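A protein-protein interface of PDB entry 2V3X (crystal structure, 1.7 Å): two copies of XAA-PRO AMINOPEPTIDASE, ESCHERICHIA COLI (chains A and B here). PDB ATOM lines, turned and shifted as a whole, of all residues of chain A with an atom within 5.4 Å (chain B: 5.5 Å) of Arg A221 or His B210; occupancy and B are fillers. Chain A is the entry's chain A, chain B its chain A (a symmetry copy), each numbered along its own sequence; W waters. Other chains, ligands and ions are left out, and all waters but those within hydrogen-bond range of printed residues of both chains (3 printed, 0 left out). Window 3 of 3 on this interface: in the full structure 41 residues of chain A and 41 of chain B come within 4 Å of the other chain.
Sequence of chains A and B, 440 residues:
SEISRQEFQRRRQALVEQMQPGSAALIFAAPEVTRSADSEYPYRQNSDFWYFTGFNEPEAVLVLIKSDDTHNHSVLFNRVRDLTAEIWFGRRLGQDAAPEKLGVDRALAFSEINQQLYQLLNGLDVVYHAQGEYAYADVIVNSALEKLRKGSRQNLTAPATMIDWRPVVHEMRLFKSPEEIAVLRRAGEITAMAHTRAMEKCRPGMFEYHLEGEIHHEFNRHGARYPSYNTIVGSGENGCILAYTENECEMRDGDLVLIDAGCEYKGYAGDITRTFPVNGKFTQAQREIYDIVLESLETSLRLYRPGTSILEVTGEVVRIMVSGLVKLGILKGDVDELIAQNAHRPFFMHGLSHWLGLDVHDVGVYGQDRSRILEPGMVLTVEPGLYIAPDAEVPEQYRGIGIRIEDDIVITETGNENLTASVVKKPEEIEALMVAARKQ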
ATOM      1  N   MET A 193      17.009  -1.696  15.441  1.00  0.00           N
ATOM      2  CA  MET A 193      15.876  -0.794  15.750  1.00  0.00           C
ATOM      3  C   MET A 193      16.356   0.447  16.481  1.00  0.00           C
ATOM      4  O   MET A 193      15.849   1.564  16.245  1.00  0.00           O
ATOM      5  CB  MET A 193      14.772  -1.509  16.531  1.00  0.00           C
ATOM      6  CG  MET A 193      13.988  -2.474  15.699  1.00  0.00           C
ATOM      7  SD  MET A 193      12.535  -3.174  16.522  1.00  0.00           S
ATOM      8  CE  MET A 193      13.307  -4.406  17.534  1.00  0.00           C
ATOM      9  N   ARG A 197      16.162   4.334  15.191  1.00  0.00           N
ATOM     10  CA  ARG A 197      15.598   5.363  16.060  1.00  0.00           C
ATOM     11  C   ARG A 197      16.541   6.552  16.205  1.00  0.00           C
ATOM     12  O   ARG A 197      16.100   7.709  16.163  1.00  0.00           O
ATOM     13  CB  ARG A 197      15.278   4.758  17.426  1.00  0.00           C
ATOM     14  CG  ARG A 197      14.733   5.762  18.437  1.00  0.00           C
ATOM     15  CD  ARG A 197      14.286   5.033  19.667  1.00  0.00           C
ATOM     16  NE  ARG A 197      13.917   5.950  20.734  1.00  0.00           N
ATOM     17  CZ  ARG A 197      13.413   5.589  21.910  1.00  0.00           C
ATOM     18  NH1 ARG A 197      13.092   4.330  22.131  1.00  0.00           N
ATOM     19  NH2 ARG A 197      13.169   6.520  22.838  1.00  0.00           N
ATOM     20  N   HIS A 216      19.501   3.468  24.314  1.00  0.00           N
ATOM     21  CA  HIS A 216      19.303   2.651  25.504  1.00  0.00           C
ATOM     22  C   HIS A 216      17.823   2.387  25.830  1.00  0.00           C
ATOM     23  O   HIS A 216      17.478   1.290  26.308  1.00  0.00           O
ATOM     24  CB  HIS A 216      20.007   3.260  26.695  1.00  0.00           C
ATOM     25  CG  HIS A 216      21.489   3.289  26.557  1.00  0.00           C
ATOM     26  ND1 HIS A 216      22.284   3.908  27.493  1.00  0.00           N
ATOM     27  CD2 HIS A 216      22.322   2.787  25.619  1.00  0.00           C
ATOM     28  CE1 HIS A 216      23.556   3.766  27.142  1.00  0.00           C
ATOM     29  NE2 HIS A 216      23.606   3.103  26.004  1.00  0.00           N
ATOM     30  N   HIS A 217      16.967   3.368  25.570  1.00  0.00           N
ATOM     31  CA  HIS A 217      15.522   3.212  25.782  1.00  0.00           C
ATOM     32  C   HIS A 217      14.982   2.150  24.834  1.00  0.00           C
ATOM     33  O   HIS A 217      14.186   1.282  25.232  1.00  0.00           O
ATOM     34  CB  HIS A 217      14.798   4.535  25.601  1.00  0.00           C
ATOM     35  CG  HIS A 217      13.333   4.456  25.887  1.00  0.00           C
ATOM     36  ND1 HIS A 217      12.409   4.105  24.919  1.00  0.00           N
ATOM     37  CD2 HIS A 217      12.632   4.643  27.027  1.00  0.00           C
ATOM     38  CE1 HIS A 217      11.199   4.112  25.454  1.00  0.00           C
ATOM     39  NE2 HIS A 217      11.306   4.439  26.730  1.00  0.00           N
ATOM     40  N   GLU A 218      15.451   2.180  23.592  1.00  0.00           N
ATOM     41  CA  GLU A 218      15.005   1.181  22.612  1.00  0.00           C
ATOM     42  C   GLU A 218      15.473  -0.232  22.999  1.00  0.00           C
ATOM     43  O   GLU A 218      14.697  -1.197  22.931  1.00  0.00           O
ATOM     44  CB  GLU A 218      15.495   1.507  21.222  1.00  0.00           C
ATOM     45  CG  GLU A 218      14.802   0.651  20.118  1.00  0.00           C
ATOM     46  CD  GLU A 218      13.315   0.970  19.923  1.00  0.00           C
ATOM     47  OE1 GLU A 218      12.802   2.012  20.400  1.00  0.00           O
ATOM     48  OE2 GLU A 218      12.631   0.153  19.247  1.00  0.00           O
ATOM     49  N   PHE A 219      16.727  -0.370  23.419  1.00  0.00           N
ATOM     50  CA  PHE A 219      17.191  -1.662  23.933  1.00  0.00           C
ATOM     51  C   PHE A 219      16.261  -2.166  25.029  1.00  0.00           C
ATOM     52  O   PHE A 219      15.806  -3.305  24.987  1.00  0.00           O
ATOM     53  CB  PHE A 219      18.584  -1.580  24.557  1.00  0.00           C
ATOM     54  CG  PHE A 219      19.728  -1.276  23.610  1.00  0.00           C
ATOM     55  CD1 PHE A 219      19.615  -1.290  22.223  1.00  0.00           C
ATOM     56  CD2 PHE A 219      20.979  -1.003  24.174  1.00  0.00           C
ATOM     57  CE1 PHE A 219      20.740  -1.028  21.408  1.00  0.00           C
ATOM     58  CE2 PHE A 219      22.075  -0.716  23.383  1.00  0.00           C
ATOM     59  CZ  PHE A 219      21.965  -0.736  21.997  1.00  0.00           C
ATOM     60  N   ASN A 220      15.985  -1.299  26.009  1.00  0.00           N
ATOM     61  CA  ASN A 220      15.160  -1.653  27.153  1.00  0.00           C
ATOM     62  C   ASN A 220      13.789  -2.128  26.794  1.00  0.00           C
ATOM     63  O   ASN A 220      13.314  -3.124  27.330  1.00  0.00           O
ATOM     64  CB  ASN A 220      15.098  -0.462  28.116  1.00  0.00           C
ATOM     65  CG  ASN A 220      14.134  -0.674  29.255  1.00  0.00           C
ATOM     66  OD1 ASN A 220      12.924  -0.529  29.067  1.00  0.00           O
ATOM     67  ND2 ASN A 220      14.664  -0.990  30.444  1.00  0.00           N
ATOM     68  N   ARG A 221      13.154  -1.450  25.851  1.00  0.00           N
ATOM     69  CA  ARG A 221      11.776  -1.773  25.580  1.00  0.00           C
ATOM     70  C   ARG A 221      11.597  -3.164  24.953  1.00  0.00           C
ATOM     71  O   ARG A 221      10.506  -3.749  25.058  1.00  0.00           O
ATOM     72  CB  ARG A 221      11.102  -0.653  24.819  1.00  0.00           C
ATOM     73  CG  ARG A 221      11.384  -0.574  23.409  1.00  0.00           C
ATOM     74  CD  ARG A 221      10.644   0.629  22.841  1.00  0.00           C
ATOM     75  NE  ARG A 221      10.538   0.514  21.406  1.00  0.00           N
ATOM     76  CZ  ARG A 221       9.577  -0.143  20.768  1.00  0.00           C
ATOM     77  NH1 ARG A 221       8.573  -0.710  21.423  1.00  0.00           N
ATOM     78  NH2 ARG A 221       9.615  -0.199  19.445  1.00  0.00           N
ATOM     79  N   HIS A 222      12.673  -3.708  24.377  1.00  0.00           N
ATOM     80  CA  HIS A 222      12.655  -5.057  23.809  1.00  0.00           C
ATOM     81  C   HIS A 222      13.243  -6.092  24.762  1.00  0.00           C
ATOM     82  O   HIS A 222      13.377  -7.255  24.397  1.00  0.00           O
ATOM     83  CB  HIS A 222      13.367  -5.104  22.464  1.00  0.00           C
ATOM     84  CG  HIS A 222      12.767  -4.183  21.466  1.00  0.00           C
ATOM     85  ND1 HIS A 222      11.493  -4.368  20.960  1.00  0.00           N
ATOM     86  CD2 HIS A 222      13.223  -3.023  20.941  1.00  0.00           C
ATOM     87  CE1 HIS A 222      11.217  -3.374  20.135  1.00  0.00           C
ATOM     88  NE2 HIS A 222      12.249  -2.550  20.100  1.00  0.00           N
ATOM     89  N   GLY A 223      13.571  -5.693  25.980  1.00  0.00           N
ATOM     90  CA  GLY A 223      14.012  -6.635  26.981  1.00  0.00           C
ATOM     91  C   GLY A 223      15.502  -6.818  27.065  1.00  0.00           C
ATOM     92  O   GLY A 223      15.963  -7.762  27.713  1.00  0.00           O
ATOM     93  N   GLY B 205       0.496  -4.957  32.509  1.00  0.00           N
ATOM     94  CA  GLY B 205       1.067  -5.723  31.403  1.00  0.00           C
ATOM     95  C   GLY B 205       2.447  -5.280  30.965  1.00  0.00           C
ATOM     96  O   GLY B 205       3.186  -6.045  30.309  1.00  0.00           O
ATOM     97  N   MET B 206       2.793  -4.037  31.270  1.00  0.00           N
ATOM     98  CA  MET B 206       4.174  -3.615  31.114  1.00  0.00           C
ATOM     99  C   MET B 206       5.032  -4.369  32.113  1.00  0.00           C
ATOM    100  O   MET B 206       4.577  -4.765  33.185  1.00  0.00           O
ATOM    101  CB  MET B 206       4.291  -2.104  31.337  1.00  0.00           C
ATOM    102  CG  MET B 206       3.738  -1.330  30.135  1.00  0.00           C
ATOM    103  SD  MET B 206       3.681   0.436  30.448  1.00  0.00           S
ATOM    104  CE  MET B 206       5.176   0.624  31.372  1.00  0.00           C
ATOM    105  N   PHE B 207       6.302  -4.544  31.772  1.00  0.00           N
ATOM    106  CA  PHE B 207       7.257  -5.129  32.699  1.00  0.00           C
ATOM    107  C   PHE B 207       7.842  -4.060  33.612  1.00  0.00           C
ATOM    108  O   PHE B 207       7.915  -2.865  33.268  1.00  0.00           O
ATOM    109  CB  PHE B 207       8.357  -5.855  31.929  1.00  0.00           C
ATOM    110  CG  PHE B 207       7.920  -7.198  31.421  1.00  0.00           C
ATOM    111  CD1 PHE B 207       7.097  -7.299  30.304  1.00  0.00           C
ATOM    112  CD2 PHE B 207       8.253  -8.342  32.112  1.00  0.00           C
ATOM    113  CE1 PHE B 207       6.653  -8.540  29.864  1.00  0.00           C
ATOM    114  CE2 PHE B 207       7.815  -9.574  31.682  1.00  0.00           C
ATOM    115  CZ  PHE B 207       7.018  -9.676  30.555  1.00  0.00           C
ATOM    116  N   GLU B 208       8.259  -4.486  34.806  1.00  0.00           N
ATOM    117  CA  GLU B 208       8.921  -3.585  35.742  1.00  0.00           C
ATOM    118  C   GLU B 208      10.070  -2.843  35.057  1.00  0.00           C
ATOM    119  O   GLU B 208      10.191  -1.645  35.215  1.00  0.00           O
ATOM    120  CB  GLU B 208       9.436  -4.379  36.946  1.00  0.00           C
ATOM    121  CG  GLU B 208       8.304  -4.879  37.858  1.00  0.00           C
ATOM    122  CD  GLU B 208       8.733  -5.996  38.812  1.00  0.00           C
ATOM    123  OE1 GLU B 208       9.720  -6.708  38.535  1.00  0.00           O
ATOM    124  OE2 GLU B 208       8.020  -6.187  39.824  1.00  0.00           O
ATOM    125  N   TYR B 209      10.878  -3.551  34.259  1.00  0.00           N
ATOM    126  CA  TYR B 209      12.009  -2.916  33.580  1.00  0.00           C
ATOM    127  C   TYR B 209      11.609  -1.828  32.587  1.00  0.00           C
ATOM    128  O   TYR B 209      12.401  -0.940  32.312  1.00  0.00           O
ATOM    129  CB  TYR B 209      12.944  -3.926  32.923  1.00  0.00           C
ATOM    130  CG  TYR B 209      12.381  -4.751  31.818  1.00  0.00           C
ATOM    131  CD1 TYR B 209      12.235  -4.239  30.523  1.00  0.00           C
ATOM    132  CD2 TYR B 209      12.020  -6.073  32.027  1.00  0.00           C
ATOM    133  CE1 TYR B 209      11.751  -5.022  29.481  1.00  0.00           C
ATOM    134  CE2 TYR B 209      11.513  -6.840  31.010  1.00  0.00           C
ATOM    135  CZ  TYR B 209      11.389  -6.327  29.724  1.00  0.00           C
ATOM    136  OH  TYR B 209      10.889  -7.113  28.701  1.00  0.00           O
ATOM    137  N   HIS B 210      10.388  -1.869  32.056  1.00  0.00           N
ATOM    138  CA  HIS B 210       9.929  -0.786  31.191  1.00  0.00           C
ATOM    139  C   HIS B 210       9.908   0.567  31.901  1.00  0.00           C
ATOM    140  O   HIS B 210      10.239   1.587  31.296  1.00  0.00           O
ATOM    141  CB  HIS B 210       8.571  -1.090  30.577  1.00  0.00           C
ATOM    142  CG  HIS B 210       8.625  -2.119  29.503  1.00  0.00           C
ATOM    143  ND1 HIS B 210       7.737  -3.166  29.429  1.00  0.00           N
ATOM    144  CD2 HIS B 210       9.465  -2.262  28.449  1.00  0.00           C
ATOM    145  CE1 HIS B 210       8.014  -3.905  28.371  1.00  0.00           C
ATOM    146  NE2 HIS B 210       9.060  -3.380  27.757  1.00  0.00           N
ATOM    147  N   LEU B 211       9.518   0.586  33.175  1.00  0.00           N
ATOM    148  CA  LEU B 211       9.512   1.827  33.919  1.00  0.00           C
ATOM    149  C   LEU B 211      10.928   2.299  34.218  1.00  0.00           C
ATOM    150  O   LEU B 211      11.194   3.493  34.217  1.00  0.00           O
ATOM    151  CB  LEU B 211       8.697   1.714  35.204  1.00  0.00           C
ATOM    152  CG  LEU B 211       7.220   1.370  35.007  1.00  0.00           C
ATOM    153  CD1 LEU B 211       6.479   1.461  36.344  1.00  0.00           C
ATOM    154  CD2 LEU B 211       6.584   2.287  33.993  1.00  0.00           C
ATOM    155  N   GLU B 212      11.844   1.359  34.454  1.00  0.00           N
ATOM    156  CA  GLU B 212      13.258   1.694  34.557  1.00  0.00           C
ATOM    157  C   GLU B 212      13.719   2.409  33.267  1.00  0.00           C
ATOM    158  O   GLU B 212      14.422   3.433  33.325  1.00  0.00           O
ATOM    159  CB  GLU B 212      14.064   0.418  34.844  1.00  0.00           C
ATOM    160  CG  GLU B 212      15.560   0.525  34.623  1.00  0.00           C
ATOM    161  CD  GLU B 212      16.261  -0.818  34.794  1.00  0.00           C
ATOM    162  OE1 GLU B 212      15.745  -1.682  35.538  1.00  0.00           O
ATOM    163  OE2 GLU B 212      17.318  -1.026  34.148  1.00  0.00           O
ATOM    164  N   GLY B 213      13.311   1.876  32.120  1.00  0.00           N
ATOM    165  CA  GLY B 213      13.671   2.478  30.835  1.00  0.00           C
ATOM    166  C   GLY B 213      13.169   3.906  30.713  1.00  0.00           C
ATOM    167  O   GLY B 213      13.890   4.778  30.242  1.00  0.00           O
ATOM    168  N   GLU B 214      11.914   4.136  31.072  1.00  0.00           N
ATOM    169  CA  GLU B 214      11.352   5.502  31.028  1.00  0.00           C
ATOM    170  C   GLU B 214      12.136   6.458  31.927  1.00  0.00           C
ATOM    171  O   GLU B 214      12.475   7.558  31.534  1.00  0.00           O
ATOM    172  CB  GLU B 214       9.884   5.501  31.464  1.00  0.00           C
ATOM    173  CG  GLU B 214       8.948   4.726  30.551  1.00  0.00           C
ATOM    174  CD  GLU B 214       8.876   5.255  29.135  1.00  0.00           C
ATOM    175  OE1 GLU B 214       8.728   6.467  28.974  1.00  0.00           O
ATOM    176  OE2 GLU B 214       8.900   4.440  28.178  1.00  0.00           O
ATOM    177  N   ILE B 215      12.420   6.010  33.158  1.00  0.00           N
ATOM    178  CA  ILE B 215      13.165   6.794  34.149  1.00  0.00           C
ATOM    179  C   ILE B 215      14.565   7.138  33.648  1.00  0.00           C
ATOM    180  O   ILE B 215      14.983   8.297  33.683  1.00  0.00           O
ATOM    181  CB  ILE B 215      13.209   6.034  35.490  1.00  0.00           C
ATOM    182  CG1 ILE B 215      11.805   6.046  36.106  1.00  0.00           C
ATOM    183  CG2 ILE B 215      14.252   6.652  36.454  1.00  0.00           C
ATOM    184  CD1 ILE B 215      11.619   5.060  37.198  1.00  0.00           C
HETATM  185  O   HOH W   1      16.256   3.923  28.929  1.00  0.00           O
HETATM  186  O   HOH W   2      17.424  -0.620  31.112  1.00  0.00           O
HETATM  187  O   HOH W   3       9.825  -6.233  26.280  1.00  0.00           O
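NE2 of His A217 sits at hydrogen-bond distance from OE2 of Glu B214, 2.8 Å away. O of Tyr B209 sits at hydrogen-bond distance from ND2 of Asn A220, 2.9 Å away. O of Arg A221 lies within hydrogen-bond range of NE2 of His B210 (3.1 Å).
The guanidinium group of Arg A197 lies within hydrogen-bond range of a ring nitrogen (ND1) of His A217 (2.9 Å). OE1 of Glu A218 is in salt-bridge range of NE of Arg A221 (2.9 Å). The backbone NH of Phe B207 is in hydrogen-bond range of a ring nitrogen (ND1) of His B210, at 3.1 Å.
Gly B213 touches His A217 (O to CD2, 3.5 Å). His B210 touches Asn A220 (CA to OD1, 3.7 Å). CA of Gly B213 touches CG of Asn A220 (3.6 Å). Gly A223 touches Tyr B209 (CA to OH, 3.6 Å).
Printed residues of chain B within 4 Å of His A217: Gly B213 and Glu B214. Printed residues of chain B within 4 Å of Asn A220: Tyr B209 (2.9 Å), His B210 (3.7 Å) and Gly B213 (3.6 Å). Printed residues of chain B within 4 Å of Arg A221: His B210 (3.1 Å). Of the printed residues of chain B, Gly A223 touches Tyr B209 (3.6 Å). Met B206 touches none of the printed residues of chain A. Phe B207 touches none of the printed residues of chain A. Of the printed residues of chain A, Tyr B209 touches Asn A220 and Gly A223. Printed residues of chain A within 4 Å of His B210: Asn A220 and Arg A221. Of the printed residues of chain A, Gly B213 touches His A217 (3.5 Å) and Asn A220 (3.6 Å).
Hydrophobic or aromatic side chains of chain B within 4 Å of the printed part of chain A: Tyr B209 and His B210. Hydrophobic or aromatic side chains of chain A that line the printed part of chain B: His A217. Among the printed residues, no Asp or Glu carboxylate lies within 4 Å of a Lys or Arg side-chain nitrogen of the other chain.
No position is printed for both chains. Of the 7 pairs that touch across the chains among the printed residues, none has its exchanged pair printed and touching as well.
Water W3 lies within hydrogen-bond range of OH of Tyr B209, O of Arg A221 and NE2 of His B210. Water W1 lies within hydrogen-bond range of the backbone carbonyl oxygen (O) of Gly B213 and the backbone NH (N) of His A217. Water W2 bridges the side-chain amide nitrogen of Asn A220 (2.9 Å) and the side-chain carboxylate of Glu B212 (3.1 Å).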
